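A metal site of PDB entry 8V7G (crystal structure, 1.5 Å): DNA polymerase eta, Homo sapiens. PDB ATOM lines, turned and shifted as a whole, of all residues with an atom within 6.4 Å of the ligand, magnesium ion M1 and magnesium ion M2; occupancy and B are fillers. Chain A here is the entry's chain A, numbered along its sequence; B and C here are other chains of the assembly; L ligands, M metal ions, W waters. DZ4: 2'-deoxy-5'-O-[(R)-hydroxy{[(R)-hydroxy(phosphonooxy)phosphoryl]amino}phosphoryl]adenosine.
Lys 234 touches magnesium ion M1. Within 4 Å of magnesium ion M1: Asp 16, Met 17, Asp 118 and Lys 234.
A nitrogen (N1) of the ligand sits close to N1 of DG 5 of chain C. Asp 18 touches the ligand (CA to O2G, 3.3 Å). Ile 51 touches the ligand (O to C2', 3.3 Å). CB of Ala 52 touches O3' of the ligand (3.6 Å). Ile 117 touches the ligand (CG2 to O4', 3.8 Å). 17 residues have an atom within 4 Å of the ligand: Asp 16, Met 17, Asp 18, Cys 19, Phe 20, Phe 21, Ile 51, Ala 52, Tyr 55, Arg 58, Arg 64, Ile 117, Asp 118, Lys 234, U7B 8 of chain B, DT 4 of chain C and DG 5 of chain C.
The backbone carbonyl oxygen of Asp 16 lies within hydrogen-bond range of the side-chain amino group of Lys 234, at 3.0 Å. The backbone NH (N) of Asp 118 sits close to the side-chain hydroxyl (OG) of Ser 116 (3.2 Å). O2 of U7B 8 of chain B sits close to N2 of DG 5 of chain C (2.7 Å). O3' of U7B 8 of chain B sits close to the side-chain hydroxyl (OG) of Ser 116 (2.9 Å). OP1 of U7B 8 of chain B is in salt-bridge range of the side-chain amino group (NZ) of Lys 227 (3.2 Å). O2 of DT 4 of chain C lies within hydrogen-bond range of the side-chain amide nitrogen of Gln 41 (3.2 Å). The backbone carbonyl oxygen of Val 53 sits at hydrogen-bond distance from the guanidinium group of Arg 58, 2.9 Å away. OD1 of Asp 18 is in salt-bridge range of NZ of Lys 234 (2.8 Å).
Ser 116 touches magnesium ion M2. Five residues have an atom within 4 Å of magnesium ion M2: Asp 16, Ser 116, Asp 118, Glu 119 and U7B 8 of chain B.
Water W9 lies within hydrogen-bond range of an oxygen (O2A) of the ligand (3.1 Å), the side-chain amino group of Lys 227 (3.1 Å) and O5' of U7B 8 of chain B (3.3 Å). Water W1 lies within hydrogen-bond range of O2B of the ligand (2.7 Å), N of Val 53 (2.8 Å) and NH2 of Arg 58 (2.9 Å). Water W8 bridges an oxygen (O3G) of the ligand (2.7 Å) and the guanidinium group (NH1) of Arg 58 (3.5 Å). Water W5 lies within hydrogen-bond range of a nitrogen (N7) of the ligand and the guanidinium group of Arg 64. Water W7 lies within hydrogen-bond range of NH1 of Arg 64 (2.7 Å), N3A of the ligand (3.1 Å) and O of Ile 51 (3.2 Å).
Magnesium ion M1 is bound by the side-chain carboxylate (OD1) of Asp 16 (2.0 Å), the side-chain carboxylate (OD2) of Asp 118 (2.0 Å), an oxygen (O1G) of the ligand (2.1 Å), an oxygen (O1B) of the ligand (2.1 Å), the backbone carbonyl oxygen (O) of Met 17 (2.1 Å) and an oxygen (O1A) of the ligand (2.2 Å).
A nitrogen (N6) of the ligand is in hydrogen-bond range of N4 of U7B 8 of chain B. The side-chain hydroxyl of Tyr 55 is in hydrogen-bond range of an oxygen (O2G) of the ligand. A nitrogen (N6) of the ligand lies within hydrogen-bond range of O4 of DT 4 of chain C (3.1 Å). The backbone NH (N) of Cys 19 lies within hydrogen-bond range of an oxygen (O2G) of the ligand. The guanidinium group of Arg 58 is in salt-bridge range of an oxygen (O3G) of the ligand. The side-chain amino group (NZ) of Lys 234 is in salt-bridge range of an oxygen (O2G) of the ligand, at 3.2 Å. O2B of the ligand is in hydrogen-bond range of N of Phe 20 (3.3 Å). The backbone NH (N) of Phe 21 sits at hydrogen-bond distance from an oxygen (O3') of the ligand (3.1 Å). NH1 of Arg 64 lies within salt-bridge range of O2A of the ligand (3.99 Å).
The side-chain carboxylate (OD2) of Asp 16 binds magnesium ion M2 (2.1 Å). OE2 of Glu 119 binds magnesium ion M2, 2.2 Å away. O3' of U7B 8 of chain B is bound to magnesium ion M2, 2.2 Å away. OD1 of Asp 118 binds magnesium ion M2, 2.2 Å away. Magnesium ion M2 is bound by water W9. O1A of the ligand binds magnesium ion M2 (2.2 Å).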
ATOM      1  N   ASP A  16       5.003 -31.857 -27.529  1.00  0.00           N
ATOM      2  CA  ASP A  16       4.082 -30.732 -27.360  1.00  0.00           C
ATOM      3  C   ASP A  16       4.638 -29.731 -26.362  1.00  0.00           C
ATOM      4  O   ASP A  16       4.903 -30.078 -25.210  1.00  0.00           O
ATOM      5  CB  ASP A  16       2.688 -31.216 -26.933  1.00  0.00           C
ATOM      6  CG  ASP A  16       1.659 -30.122 -27.001  1.00  0.00           C
ATOM      7  OD1 ASP A  16       1.764 -29.207 -26.172  1.00  0.00           O
ATOM      8  OD2 ASP A  16       0.808 -30.109 -27.911  1.00  0.00           O
ATOM      9  N   MET A  17       4.708 -28.474 -26.793  1.00  0.00           N
ATOM     10  CA  MET A  17       5.331 -27.476 -25.942  1.00  0.00           C
ATOM     11  C   MET A  17       4.414 -27.211 -24.751  1.00  0.00           C
ATOM     12  O   MET A  17       3.184 -27.205 -24.870  1.00  0.00           O
ATOM     13  CB  MET A  17       5.583 -26.176 -26.747  1.00  0.00           C
ATOM     14  CG  MET A  17       6.446 -26.435 -27.995  1.00  0.00           C
ATOM     15  SD  MET A  17       8.043 -27.215 -27.709  1.00  0.00           S
ATOM     16  CE  MET A  17       8.912 -26.113 -26.651  1.00  0.00           C
ATOM     17  N   ASP A  18       5.015 -27.025 -23.577  1.00  0.00           N
ATOM     18  CA  ASP A  18       4.233 -26.668 -22.396  1.00  0.00           C
ATOM     19  C   ASP A  18       3.816 -25.206 -22.448  1.00  0.00           C
ATOM     20  O   ASP A  18       4.631 -24.342 -22.779  1.00  0.00           O
ATOM     21  CB  ASP A  18       5.009 -26.952 -21.106  1.00  0.00           C
ATOM     22  CG  ASP A  18       5.396 -28.420 -20.955  1.00  0.00           C
ATOM     23  OD1 ASP A  18       4.691 -29.296 -21.480  1.00  0.00           O
ATOM     24  OD2 ASP A  18       6.409 -28.691 -20.297  1.00  0.00           O
ATOM     25  N   CYS A  19       2.534 -24.938 -22.167  1.00  0.00           N
ATOM     26  CA  CYS A  19       1.935 -23.593 -22.141  1.00  0.00           C
ATOM     27  C   CYS A  19       2.657 -22.660 -23.109  1.00  0.00           C
ATOM     28  O   CYS A  19       3.253 -21.647 -22.697  1.00  0.00           O
ATOM     29  CB  CYS A  19       1.892 -23.027 -20.712  1.00  0.00           C
ATOM     30  SG  CYS A  19       3.384 -22.986 -19.727  1.00  0.00           S
ATOM     31  N   PHE A  20       2.618 -22.984 -24.401  1.00  0.00           N
ATOM     32  CA  PHE A  20       3.643 -22.499 -25.342  1.00  0.00           C
ATOM     33  C   PHE A  20       3.701 -20.976 -25.430  1.00  0.00           C
ATOM     34  O   PHE A  20       4.775 -20.388 -25.252  1.00  0.00           O
ATOM     35  CB  PHE A  20       3.402 -23.100 -26.727  1.00  0.00           C
ATOM     36  CG  PHE A  20       4.429 -22.694 -27.730  1.00  0.00           C
ATOM     37  CD1 PHE A  20       5.804 -22.769 -27.424  1.00  0.00           C
ATOM     38  CD2 PHE A  20       4.056 -22.246 -28.992  1.00  0.00           C
ATOM     39  CE1 PHE A  20       6.772 -22.392 -28.365  1.00  0.00           C
ATOM     40  CE2 PHE A  20       5.038 -21.884 -29.948  1.00  0.00           C
ATOM     41  CZ  PHE A  20       6.378 -21.956 -29.627  1.00  0.00           C
ATOM     42  N   PHE A  21       2.579 -20.314 -25.723  1.00  0.00           N
ATOM     43  CA  PHE A  21       2.664 -18.847 -25.885  1.00  0.00           C
ATOM     44  C   PHE A  21       3.123 -18.178 -24.597  1.00  0.00           C
ATOM     45  O   PHE A  21       3.829 -17.160 -24.634  1.00  0.00           O
ATOM     46  CB  PHE A  21       1.325 -18.247 -26.325  1.00  0.00           C
ATOM     47  CG  PHE A  21       0.901 -18.565 -27.731  1.00  0.00           C
ATOM     48  CD1 PHE A  21       1.480 -19.586 -28.478  1.00  0.00           C
ATOM     49  CD2 PHE A  21      -0.163 -17.863 -28.298  1.00  0.00           C
ATOM     50  CE1 PHE A  21       1.035 -19.867 -29.795  1.00  0.00           C
ATOM     51  CE2 PHE A  21      -0.604 -18.152 -29.588  1.00  0.00           C
ATOM     52  CZ  PHE A  21      -0.007 -19.147 -30.338  1.00  0.00           C
ATOM     53  N   VAL A  22       2.727 -18.712 -23.437  1.00  0.00           N
ATOM     54  CA  VAL A  22       3.234 -18.188 -22.177  1.00  0.00           C
ATOM     55  C   VAL A  22       4.761 -18.326 -22.101  1.00  0.00           C
ATOM     56  O   VAL A  22       5.460 -17.381 -21.726  1.00  0.00           O
ATOM     57  CB  VAL A  22       2.559 -18.893 -20.992  1.00  0.00           C
ATOM     58  CG1 VAL A  22       3.317 -18.587 -19.689  1.00  0.00           C
ATOM     59  CG2 VAL A  22       1.085 -18.489 -20.886  1.00  0.00           C
ATOM     60  N   GLN A  41      -5.654 -12.028 -25.862  1.00  0.00           N
ATOM     61  CA  GLN A  41      -5.898 -11.356 -27.138  1.00  0.00           C
ATOM     62  C   GLN A  41      -6.926 -10.266 -26.924  1.00  0.00           C
ATOM     63  O   GLN A  41      -8.012 -10.539 -26.403  1.00  0.00           O
ATOM     64  CB  GLN A  41      -6.412 -12.316 -28.220  1.00  0.00           C
ATOM     65  CG  GLN A  41      -5.352 -13.102 -28.923  1.00  0.00           C
ATOM     66  CD  GLN A  41      -5.899 -13.967 -30.046  1.00  0.00           C
ATOM     67  OE1 GLN A  41      -5.224 -14.155 -31.063  1.00  0.00           O
ATOM     68  NE2 GLN A  41      -7.106 -14.491 -29.878  1.00  0.00           N
ATOM     69  N   ILE A  51      -5.725 -17.168 -24.178  1.00  0.00           N
ATOM     70  CA  ILE A  51      -5.428 -18.261 -25.088  1.00  0.00           C
ATOM     71  C   ILE A  51      -4.333 -19.203 -24.597  1.00  0.00           C
ATOM     72  O   ILE A  51      -4.174 -20.283 -25.181  1.00  0.00           O
ATOM     73  CB  ILE A  51      -5.101 -17.761 -26.508  1.00  0.00           C
ATOM     74  CG1 ILE A  51      -3.903 -16.806 -26.525  1.00  0.00           C
ATOM     75  CG2 ILE A  51      -6.360 -17.128 -27.138  1.00  0.00           C
ATOM     76  CD1 ILE A  51      -3.436 -16.493 -27.948  1.00  0.00           C
ATOM     77  N   ALA A  52      -3.606 -18.867 -23.526  1.00  0.00           N
ATOM     78  CA  ALA A  52      -2.584 -19.754 -22.955  1.00  0.00           C
ATOM     79  C   ALA A  52      -2.391 -19.398 -21.493  1.00  0.00           C
ATOM     80  O   ALA A  52      -2.517 -18.233 -21.119  1.00  0.00           O
ATOM     81  CB  ALA A  52      -1.243 -19.656 -23.704  1.00  0.00           C
ATOM     82  N   VAL A  53      -2.095 -20.414 -20.655  1.00  0.00           N
ATOM     83  CA  VAL A  53      -2.107 -20.294 -19.199  1.00  0.00           C
ATOM     84  C   VAL A  53      -0.930 -21.049 -18.607  1.00  0.00           C
ATOM     85  O   VAL A  53      -0.762 -22.247 -18.870  1.00  0.00           O
ATOM     86  CB  VAL A  53      -3.418 -20.852 -18.621  1.00  0.00           C
ATOM     87  CG1 VAL A  53      -3.480 -20.574 -17.140  1.00  0.00           C
ATOM     88  CG2 VAL A  53      -4.613 -20.234 -19.281  1.00  0.00           C
ATOM     89  N   TYR A  55       1.243 -23.019 -15.730  1.00  0.00           N
ATOM     90  CA  TYR A  55       0.765 -24.054 -14.817  1.00  0.00           C
ATOM     91  C   TYR A  55       0.494 -23.490 -13.419  1.00  0.00           C
ATOM     92  O   TYR A  55      -0.464 -23.918 -12.748  1.00  0.00           O
ATOM     93  CB  TYR A  55       1.751 -25.238 -14.813  1.00  0.00           C
ATOM     94  CG  TYR A  55       1.550 -26.121 -16.042  1.00  0.00           C
ATOM     95  CD1 TYR A  55       2.073 -25.758 -17.296  1.00  0.00           C
ATOM     96  CD2 TYR A  55       0.746 -27.265 -15.981  1.00  0.00           C
ATOM     97  CE1 TYR A  55       1.840 -26.540 -18.438  1.00  0.00           C
ATOM     98  CE2 TYR A  55       0.509 -28.050 -17.101  1.00  0.00           C
ATOM     99  CZ  TYR A  55       1.046 -27.677 -18.325  1.00  0.00           C
ATOM    100  OH  TYR A  55       0.777 -28.472 -19.427  1.00  0.00           O
ATOM    101  N   ARG A  58      -2.912 -22.181 -13.753  1.00  0.00           N
ATOM    102  CA  ARG A  58      -3.893 -23.274 -13.827  1.00  0.00           C
ATOM    103  C   ARG A  58      -4.268 -23.789 -12.434  1.00  0.00           C
ATOM    104  O   ARG A  58      -5.415 -24.204 -12.228  1.00  0.00           O
ATOM    105  CB  ARG A  58      -3.363 -24.418 -14.686  1.00  0.00           C
ATOM    106  CG  ARG A  58      -3.179 -24.072 -16.165  1.00  0.00           C
ATOM    107  CD  ARG A  58      -2.619 -25.253 -16.920  1.00  0.00           C
ATOM    108  NE  ARG A  58      -2.003 -24.812 -18.173  1.00  0.00           N
ATOM    109  CZ  ARG A  58      -1.777 -25.575 -19.228  1.00  0.00           C
ATOM    110  NH1 ARG A  58      -2.069 -26.868 -19.220  1.00  0.00           N
ATOM    111  NH2 ARG A  58      -1.193 -25.050 -20.309  1.00  0.00           N
ATOM    112  N   ARG A  64      -7.884 -21.478 -20.692  1.00  0.00           N
ATOM    113  CA  ARG A  64      -8.084 -20.844 -22.009  1.00  0.00           C
ATOM    114  C   ARG A  64      -9.578 -20.589 -22.228  1.00  0.00           C
ATOM    115  O   ARG A  64     -10.375 -21.325 -21.629  1.00  0.00           O
ATOM    116  CB  ARG A  64      -7.528 -21.781 -23.094  1.00  0.00           C
ATOM    117  CG  ARG A  64      -7.838 -21.386 -24.524  1.00  0.00           C
ATOM    118  CD  ARG A  64      -7.331 -22.495 -25.435  1.00  0.00           C
ATOM    119  NE  ARG A  64      -8.025 -23.746 -25.192  1.00  0.00           N
ATOM    120  CZ  ARG A  64      -7.434 -24.909 -24.924  1.00  0.00           C
ATOM    121  NH1 ARG A  64      -6.121 -24.997 -24.888  1.00  0.00           N
ATOM    122  NH2 ARG A  64      -8.168 -25.987 -24.698  1.00  0.00           N
ATOM    123  N   LEU A  92       0.012 -13.157 -34.874  1.00  0.00           N
ATOM    124  CA  LEU A  92       0.621 -14.294 -34.176  1.00  0.00           C
ATOM    125  C   LEU A  92       2.080 -14.553 -34.609  1.00  0.00           C
ATOM    126  O   LEU A  92       2.623 -15.619 -34.297  1.00  0.00           O
ATOM    127  CB  LEU A  92      -0.239 -15.547 -34.384  1.00  0.00           C
ATOM    128  CG  LEU A  92      -1.722 -15.405 -33.989  1.00  0.00           C
ATOM    129  CD1 LEU A  92      -2.518 -16.657 -34.357  1.00  0.00           C
ATOM    130  CD2 LEU A  92      -1.816 -15.137 -32.491  1.00  0.00           C
ATOM    131  N   SER A 116       0.667 -28.929 -35.062  1.00  0.00           N
ATOM    132  CA  SER A 116       0.089 -27.632 -34.703  1.00  0.00           C
ATOM    133  C   SER A 116       1.242 -26.663 -34.515  1.00  0.00           C
ATOM    134  O   SER A 116       2.408 -27.042 -34.585  1.00  0.00           O
ATOM    135  CB  SER A 116      -0.770 -27.700 -33.434  1.00  0.00           C
ATOM    136  OG  SER A 116       0.046 -27.692 -32.266  1.00  0.00           O
ATOM    137  N   ILE A 117       0.899 -25.420 -34.150  1.00  0.00           N
ATOM    138  CA  ILE A 117       1.936 -24.426 -33.905  1.00  0.00           C
ATOM    139  C   ILE A 117       2.928 -24.890 -32.831  1.00  0.00           C
ATOM    140  O   ILE A 117       4.083 -24.456 -32.823  1.00  0.00           O
ATOM    141  CB  ILE A 117       1.300 -23.065 -33.540  1.00  0.00           C
ATOM    142  CG1 ILE A 117       2.331 -21.952 -33.684  1.00  0.00           C
ATOM    143  CG2 ILE A 117       0.726 -23.093 -32.127  1.00  0.00           C
ATOM    144  CD1 ILE A 117       1.719 -20.557 -33.754  1.00  0.00           C
ATOM    145  N   ASP A 118       2.512 -25.767 -31.896  1.00  0.00           N
ATOM    146  CA  ASP A 118       3.433 -26.169 -30.836  1.00  0.00           C
ATOM    147  C   ASP A 118       3.655 -27.676 -30.744  1.00  0.00           C
ATOM    148  O   ASP A 118       4.183 -28.144 -29.715  1.00  0.00           O
ATOM    149  CB  ASP A 118       2.991 -25.599 -29.483  1.00  0.00           C
ATOM    150  CG  ASP A 118       2.063 -26.522 -28.710  1.00  0.00           C
ATOM    151  OD1 ASP A 118       1.206 -27.198 -29.323  1.00  0.00           O
ATOM    152  OD2 ASP A 118       2.199 -26.584 -27.452  1.00  0.00           O
ATOM    153  N   GLU A 119       3.338 -28.450 -31.773  1.00  0.00           N
ATOM    154  CA  GLU A 119       3.584 -29.884 -31.603  1.00  0.00           C
ATOM    155  C   GLU A 119       3.893 -30.541 -32.923  1.00  0.00           C
ATOM    156  O   GLU A 119       3.399 -30.118 -33.986  1.00  0.00           O
ATOM    157  CB  GLU A 119       2.417 -30.658 -31.000  1.00  0.00           C
ATOM    158  CG  GLU A 119       1.150 -30.476 -31.755  1.00  0.00           C
ATOM    159  CD  GLU A 119      -0.073 -30.754 -30.929  1.00  0.00           C
ATOM    160  OE1 GLU A 119      -0.415 -31.915 -30.613  1.00  0.00           O
ATOM    161  OE2 GLU A 119      -0.598 -29.738 -30.453  1.00  0.00           O
ATOM    162  N   SER A 216       6.636 -31.427 -23.219  1.00  0.00           N
ATOM    163  CA  SER A 216       6.353 -32.805 -22.835  1.00  0.00           C
ATOM    164  C   SER A 216       6.297 -33.655 -24.086  1.00  0.00           C
ATOM    165  O   SER A 216       6.243 -33.152 -25.196  1.00  0.00           O
ATOM    166  CB  SER A 216       5.051 -32.899 -22.039  1.00  0.00           C
ATOM    167  OG  SER A 216       5.135 -32.065 -20.887  1.00  0.00           O
ATOM    168  N   LYS A 227       0.238 -39.183 -28.804  1.00  0.00           N
ATOM    169  CA  LYS A 227      -0.448 -37.969 -28.385  1.00  0.00           C
ATOM    170  C   LYS A 227      -1.114 -38.167 -27.022  1.00  0.00           C
ATOM    171  O   LYS A 227      -0.992 -37.309 -26.131  1.00  0.00           O
ATOM    172  CB  LYS A 227      -1.479 -37.546 -29.443  1.00  0.00           C
ATOM    173  CG  LYS A 227      -2.386 -36.404 -29.009  1.00  0.00           C
ATOM    174  CD  LYS A 227      -1.602 -35.112 -28.851  1.00  0.00           C
ATOM    175  CE  LYS A 227      -2.528 -33.961 -28.524  1.00  0.00           C
ATOM    176  NZ  LYS A 227      -1.789 -32.674 -28.345  1.00  0.00           N
ATOM    177  N   LYS A 234       2.239 -34.121 -18.308  1.00  0.00           N
ATOM    178  CA  LYS A 234       2.590 -32.714 -18.456  1.00  0.00           C
ATOM    179  C   LYS A 234       2.599 -32.024 -17.089  1.00  0.00           C
ATOM    180  O   LYS A 234       1.762 -32.326 -16.228  1.00  0.00           O
ATOM    181  CB  LYS A 234       1.555 -32.039 -19.341  1.00  0.00           C
ATOM    182  CG  LYS A 234       1.809 -32.143 -20.817  1.00  0.00           C
ATOM    183  CD  LYS A 234       1.036 -31.106 -21.615  1.00  0.00           C
ATOM    184  CE  LYS A 234       1.624 -30.977 -23.054  1.00  0.00           C
ATOM    185  NZ  LYS A 234       2.592 -29.834 -23.238  1.00  0.00           N
ATOM    186  N   PRO A 235       3.474 -31.033 -16.870  1.00  0.00           N
ATOM    187  CA  PRO A 235       4.463 -30.492 -17.826  1.00  0.00           C
ATOM    188  C   PRO A 235       5.863 -31.050 -17.623  1.00  0.00           C
ATOM    189  O   PRO A 235       6.199 -31.660 -16.589  1.00  0.00           O
ATOM    190  CB  PRO A 235       4.453 -28.998 -17.509  1.00  0.00           C
ATOM    191  CG  PRO A 235       4.248 -28.959 -16.009  1.00  0.00           C
ATOM    192  CD  PRO A 235       3.336 -30.146 -15.704  1.00  0.00           C
ATOM    193  P   U7B B   8      -5.825 -30.816 -28.981  1.00  0.00           P
ATOM    194  C5' U7B B   8      -3.879 -29.734 -30.492  1.00  0.00           C
ATOM    195  O5' U7B B   8      -4.897 -29.557 -29.505  1.00  0.00           O
ATOM    196  C4' U7B B   8      -3.641 -28.451 -31.129  1.00  0.00           C
ATOM    197  O4' U7B B   8      -4.905 -27.911 -31.577  1.00  0.00           O
ATOM    198  C3' U7B B   8      -3.180 -27.405 -30.111  1.00  0.00           C
ATOM    199  O3' U7B B   8      -1.732 -27.426 -29.965  1.00  0.00           O
ATOM    200  C2' U7B B   8      -3.610 -26.069 -30.779  1.00  0.00           C
ATOM    201  C1' U7B B   8      -4.755 -26.520 -31.809  1.00  0.00           C
ATOM    202  N1  U7B B   8      -6.041 -25.906 -31.634  1.00  0.00           N
ATOM    203  C2  U7B B   8      -6.264 -24.650 -32.158  1.00  0.00           C
ATOM    204  O2  U7B B   8      -5.354 -24.051 -32.711  1.00  0.00           O
ATOM    205  N3  U7B B   8      -7.491 -24.085 -32.060  1.00  0.00           N
ATOM    206  C4  U7B B   8      -8.484 -24.720 -31.459  1.00  0.00           C
ATOM    207  N4  U7B B   8      -9.667 -24.141 -31.371  1.00  0.00           N
ATOM    208  C5  U7B B   8      -8.277 -26.006 -30.919  1.00  0.00           C
ATOM    209  C6  U7B B   8      -7.067 -26.583 -31.026  1.00  0.00           C
ATOM    210  OP1 U7B B   8      -4.934 -31.863 -28.369  1.00  0.00           O
ATOM    211  OP2 U7B B   8      -6.861 -30.303 -28.026  1.00  0.00           O
ATOM    212  F1  U7B B   8      -2.578 -25.555 -31.497  1.00  0.00           F
ATOM    213  F2  U7B B   8      -4.008 -25.149 -29.889  1.00  0.00           F
ATOM    214  P    DT C   4     -15.233 -13.840 -30.489  1.00  0.00           P
ATOM    215  OP1  DT C   4     -15.354 -12.364 -30.517  1.00  0.00           O
ATOM    216  OP2  DT C   4     -16.049 -14.666 -31.414  1.00  0.00           O
ATOM    217  O5'  DT C   4     -13.701 -14.205 -30.705  1.00  0.00           O
ATOM    218  C5'  DT C   4     -12.694 -13.496 -30.017  1.00  0.00           C
ATOM    219  C4'  DT C   4     -11.359 -13.708 -30.692  1.00  0.00           C
ATOM    220  O4'  DT C   4     -10.825 -14.987 -30.330  1.00  0.00           O
ATOM    221  C3'  DT C   4     -11.386 -13.690 -32.220  1.00  0.00           C
ATOM    222  O3'  DT C   4     -10.270 -12.974 -32.638  1.00  0.00           O
ATOM    223  C2'  DT C   4     -11.314 -15.179 -32.606  1.00  0.00           C
ATOM    224  C1'  DT C   4     -10.439 -15.709 -31.480  1.00  0.00           C
ATOM    225  N1   DT C   4     -10.610 -17.130 -31.164  1.00  0.00           N
ATOM    226  C2   DT C   4      -9.493 -17.825 -30.813  1.00  0.00           C
ATOM    227  O2   DT C   4      -8.374 -17.326 -30.810  1.00  0.00           O
ATOM    228  N3   DT C   4      -9.702 -19.126 -30.485  1.00  0.00           N
ATOM    229  C4   DT C   4     -10.901 -19.801 -30.437  1.00  0.00           C
ATOM    230  O4   DT C   4     -10.974 -20.978 -30.110  1.00  0.00           O
ATOM    231  C5   DT C   4     -12.065 -19.013 -30.790  1.00  0.00           C
ATOM    232  C7   DT C   4     -13.424 -19.642 -30.785  1.00  0.00           C
ATOM    233  C6   DT C   4     -11.862 -17.716 -31.134  1.00  0.00           C
ATOM    234  P    DG C   5      -9.980 -12.703 -34.187  1.00  0.00           P
ATOM    235  OP1  DG C   5      -9.461 -11.329 -34.313  1.00  0.00           O
ATOM    236  OP2  DG C   5     -11.162 -13.120 -34.962  1.00  0.00           O
ATOM    237  O5'  DG C   5      -8.808 -13.742 -34.507  1.00  0.00           O
ATOM    238  C5'  DG C   5      -7.530 -13.575 -33.919  1.00  0.00           C
ATOM    239  C4'  DG C   5      -6.614 -14.666 -34.399  1.00  0.00           C
ATOM    240  O4'  DG C   5      -7.058 -15.938 -33.852  1.00  0.00           O
ATOM    241  C3'  DG C   5      -6.590 -14.858 -35.922  1.00  0.00           C
ATOM    242  O3'  DG C   5      -5.270 -15.202 -36.314  1.00  0.00           O
ATOM    243  C2'  DG C   5      -7.548 -16.026 -36.127  1.00  0.00           C
ATOM    244  C1'  DG C   5      -7.188 -16.858 -34.917  1.00  0.00           C
ATOM    245  N9   DG C   5      -8.158 -17.853 -34.561  1.00  0.00           N
ATOM    246  C8   DG C   5      -9.531 -17.783 -34.690  1.00  0.00           C
ATOM    247  N7   DG C   5     -10.149 -18.869 -34.277  1.00  0.00           N
ATOM    248  C5   DG C   5      -9.107 -19.699 -33.864  1.00  0.00           C
ATOM    249  C6   DG C   5      -9.137 -21.022 -33.333  1.00  0.00           C
ATOM    250  O6   DG C   5     -10.119 -21.744 -33.103  1.00  0.00           O
ATOM    251  N1   DG C   5      -7.857 -21.490 -33.045  1.00  0.00           N
ATOM    252  C2   DG C   5      -6.710 -20.788 -33.256  1.00  0.00           C
ATOM    253  N2   DG C   5      -5.569 -21.400 -32.921  1.00  0.00           N
ATOM    254  N3   DG C   5      -6.658 -19.564 -33.753  1.00  0.00           N
ATOM    255  C4   DG C   5      -7.902 -19.094 -34.030  1.00  0.00           C
HETATM  256  N1  DZ4 L   1      -7.355 -20.419 -29.817  1.00  0.00           N
HETATM  257  C2  DZ4 L   1      -6.233 -19.740 -30.075  1.00  0.00           C
HETATM  258  N3  DZ4 L   1      -5.020 -20.129 -29.730  1.00  0.00           N
HETATM  259  C4  DZ4 L   1      -4.939 -21.314 -29.087  1.00  0.00           C
HETATM  260  C5  DZ4 L   1      -6.070 -22.080 -28.779  1.00  0.00           C
HETATM  261  C6  DZ4 L   1      -7.311 -21.597 -29.173  1.00  0.00           C
HETATM  262  N6  DZ4 L   1      -8.446 -22.271 -28.911  1.00  0.00           N
HETATM  263  N7  DZ4 L   1      -5.642 -23.193 -28.133  1.00  0.00           N
HETATM  264  C8  DZ4 L   1      -4.292 -23.119 -28.033  1.00  0.00           C
HETATM  265  N9  DZ4 L   1      -3.874 -21.977 -28.606  1.00  0.00           N
HETATM  266  PA  DZ4 L   1      -1.781 -26.280 -26.676  1.00  0.00           P
HETATM  267  PB  DZ4 L   1      -0.397 -25.015 -24.399  1.00  0.00           P
HETATM  268  PG  DZ4 L   1      -0.080 -27.396 -22.738  1.00  0.00           P
HETATM  269  C1' DZ4 L   1      -2.463 -21.533 -28.726  1.00  0.00           C
HETATM  270  O1A DZ4 L   1      -0.665 -27.210 -26.887  1.00  0.00           O
HETATM  271  O1B DZ4 L   1       0.825 -25.334 -25.156  1.00  0.00           O
HETATM  272  O1G DZ4 L   1       0.311 -27.992 -24.060  1.00  0.00           O
HETATM  273  C2' DZ4 L   1      -1.840 -21.068 -27.414  1.00  0.00           C
HETATM  274  O2A DZ4 L   1      -3.216 -26.916 -26.832  1.00  0.00           O
HETATM  275  O2B DZ4 L   1      -0.601 -23.551 -24.007  1.00  0.00           O
HETATM  276  O2G DZ4 L   1       1.071 -27.414 -21.729  1.00  0.00           O
HETATM  277  C3' DZ4 L   1      -1.135 -22.326 -26.916  1.00  0.00           C
HETATM  278  O3' DZ4 L   1      -0.010 -21.966 -26.112  1.00  0.00           O
HETATM  279  N3A DZ4 L   1      -1.727 -25.596 -25.176  1.00  0.00           N
HETATM  280  O3B DZ4 L   1      -0.385 -25.807 -23.016  1.00  0.00           O
HETATM  281  O3G DZ4 L   1      -1.378 -27.952 -22.094  1.00  0.00           O
HETATM  282  C4' DZ4 L   1      -0.666 -22.928 -28.238  1.00  0.00           C
HETATM  283  O4' DZ4 L   1      -1.695 -22.626 -29.213  1.00  0.00           O
HETATM  284  C5' DZ4 L   1      -0.501 -24.476 -28.141  1.00  0.00           C
HETATM  285  O5' DZ4 L   1      -1.729 -25.081 -27.755  1.00  0.00           O
HETATM  286 MG    MG M   1       1.276 -27.296 -25.795  1.00  0.00          MG
HETATM  287 MG    MG M   2      -0.380 -28.532 -28.683  1.00  0.00          MG
HETATM  288  O   HOH W   1      -2.185 -22.925 -21.929  1.00  0.00           O
HETATM  289  O   HOH W   2      -3.785 -26.991 -22.403  1.00  0.00           O
HETATM  290  O   HOH W   3      -1.267 -30.073 -25.099  1.00  0.00           O
HETATM  291  O   HOH W   4      -3.439 -18.557 -31.426  1.00  0.00           O
HETATM  292  O   HOH W   5      -5.851 -26.021 -27.728  1.00  0.00           O
HETATM  293  O   HOH W   6      -2.820 -22.931 -31.837  1.00  0.00           O
HETATM  294  O   HOH W   7      -3.948 -23.436 -24.682  1.00  0.00           O
HETATM  295  O   HOH W   8      -2.279 -30.054 -20.629  1.00  0.00           O
HETATM  296  O   HOH W   9      -2.040 -29.590 -27.764  1.00  0.00           O
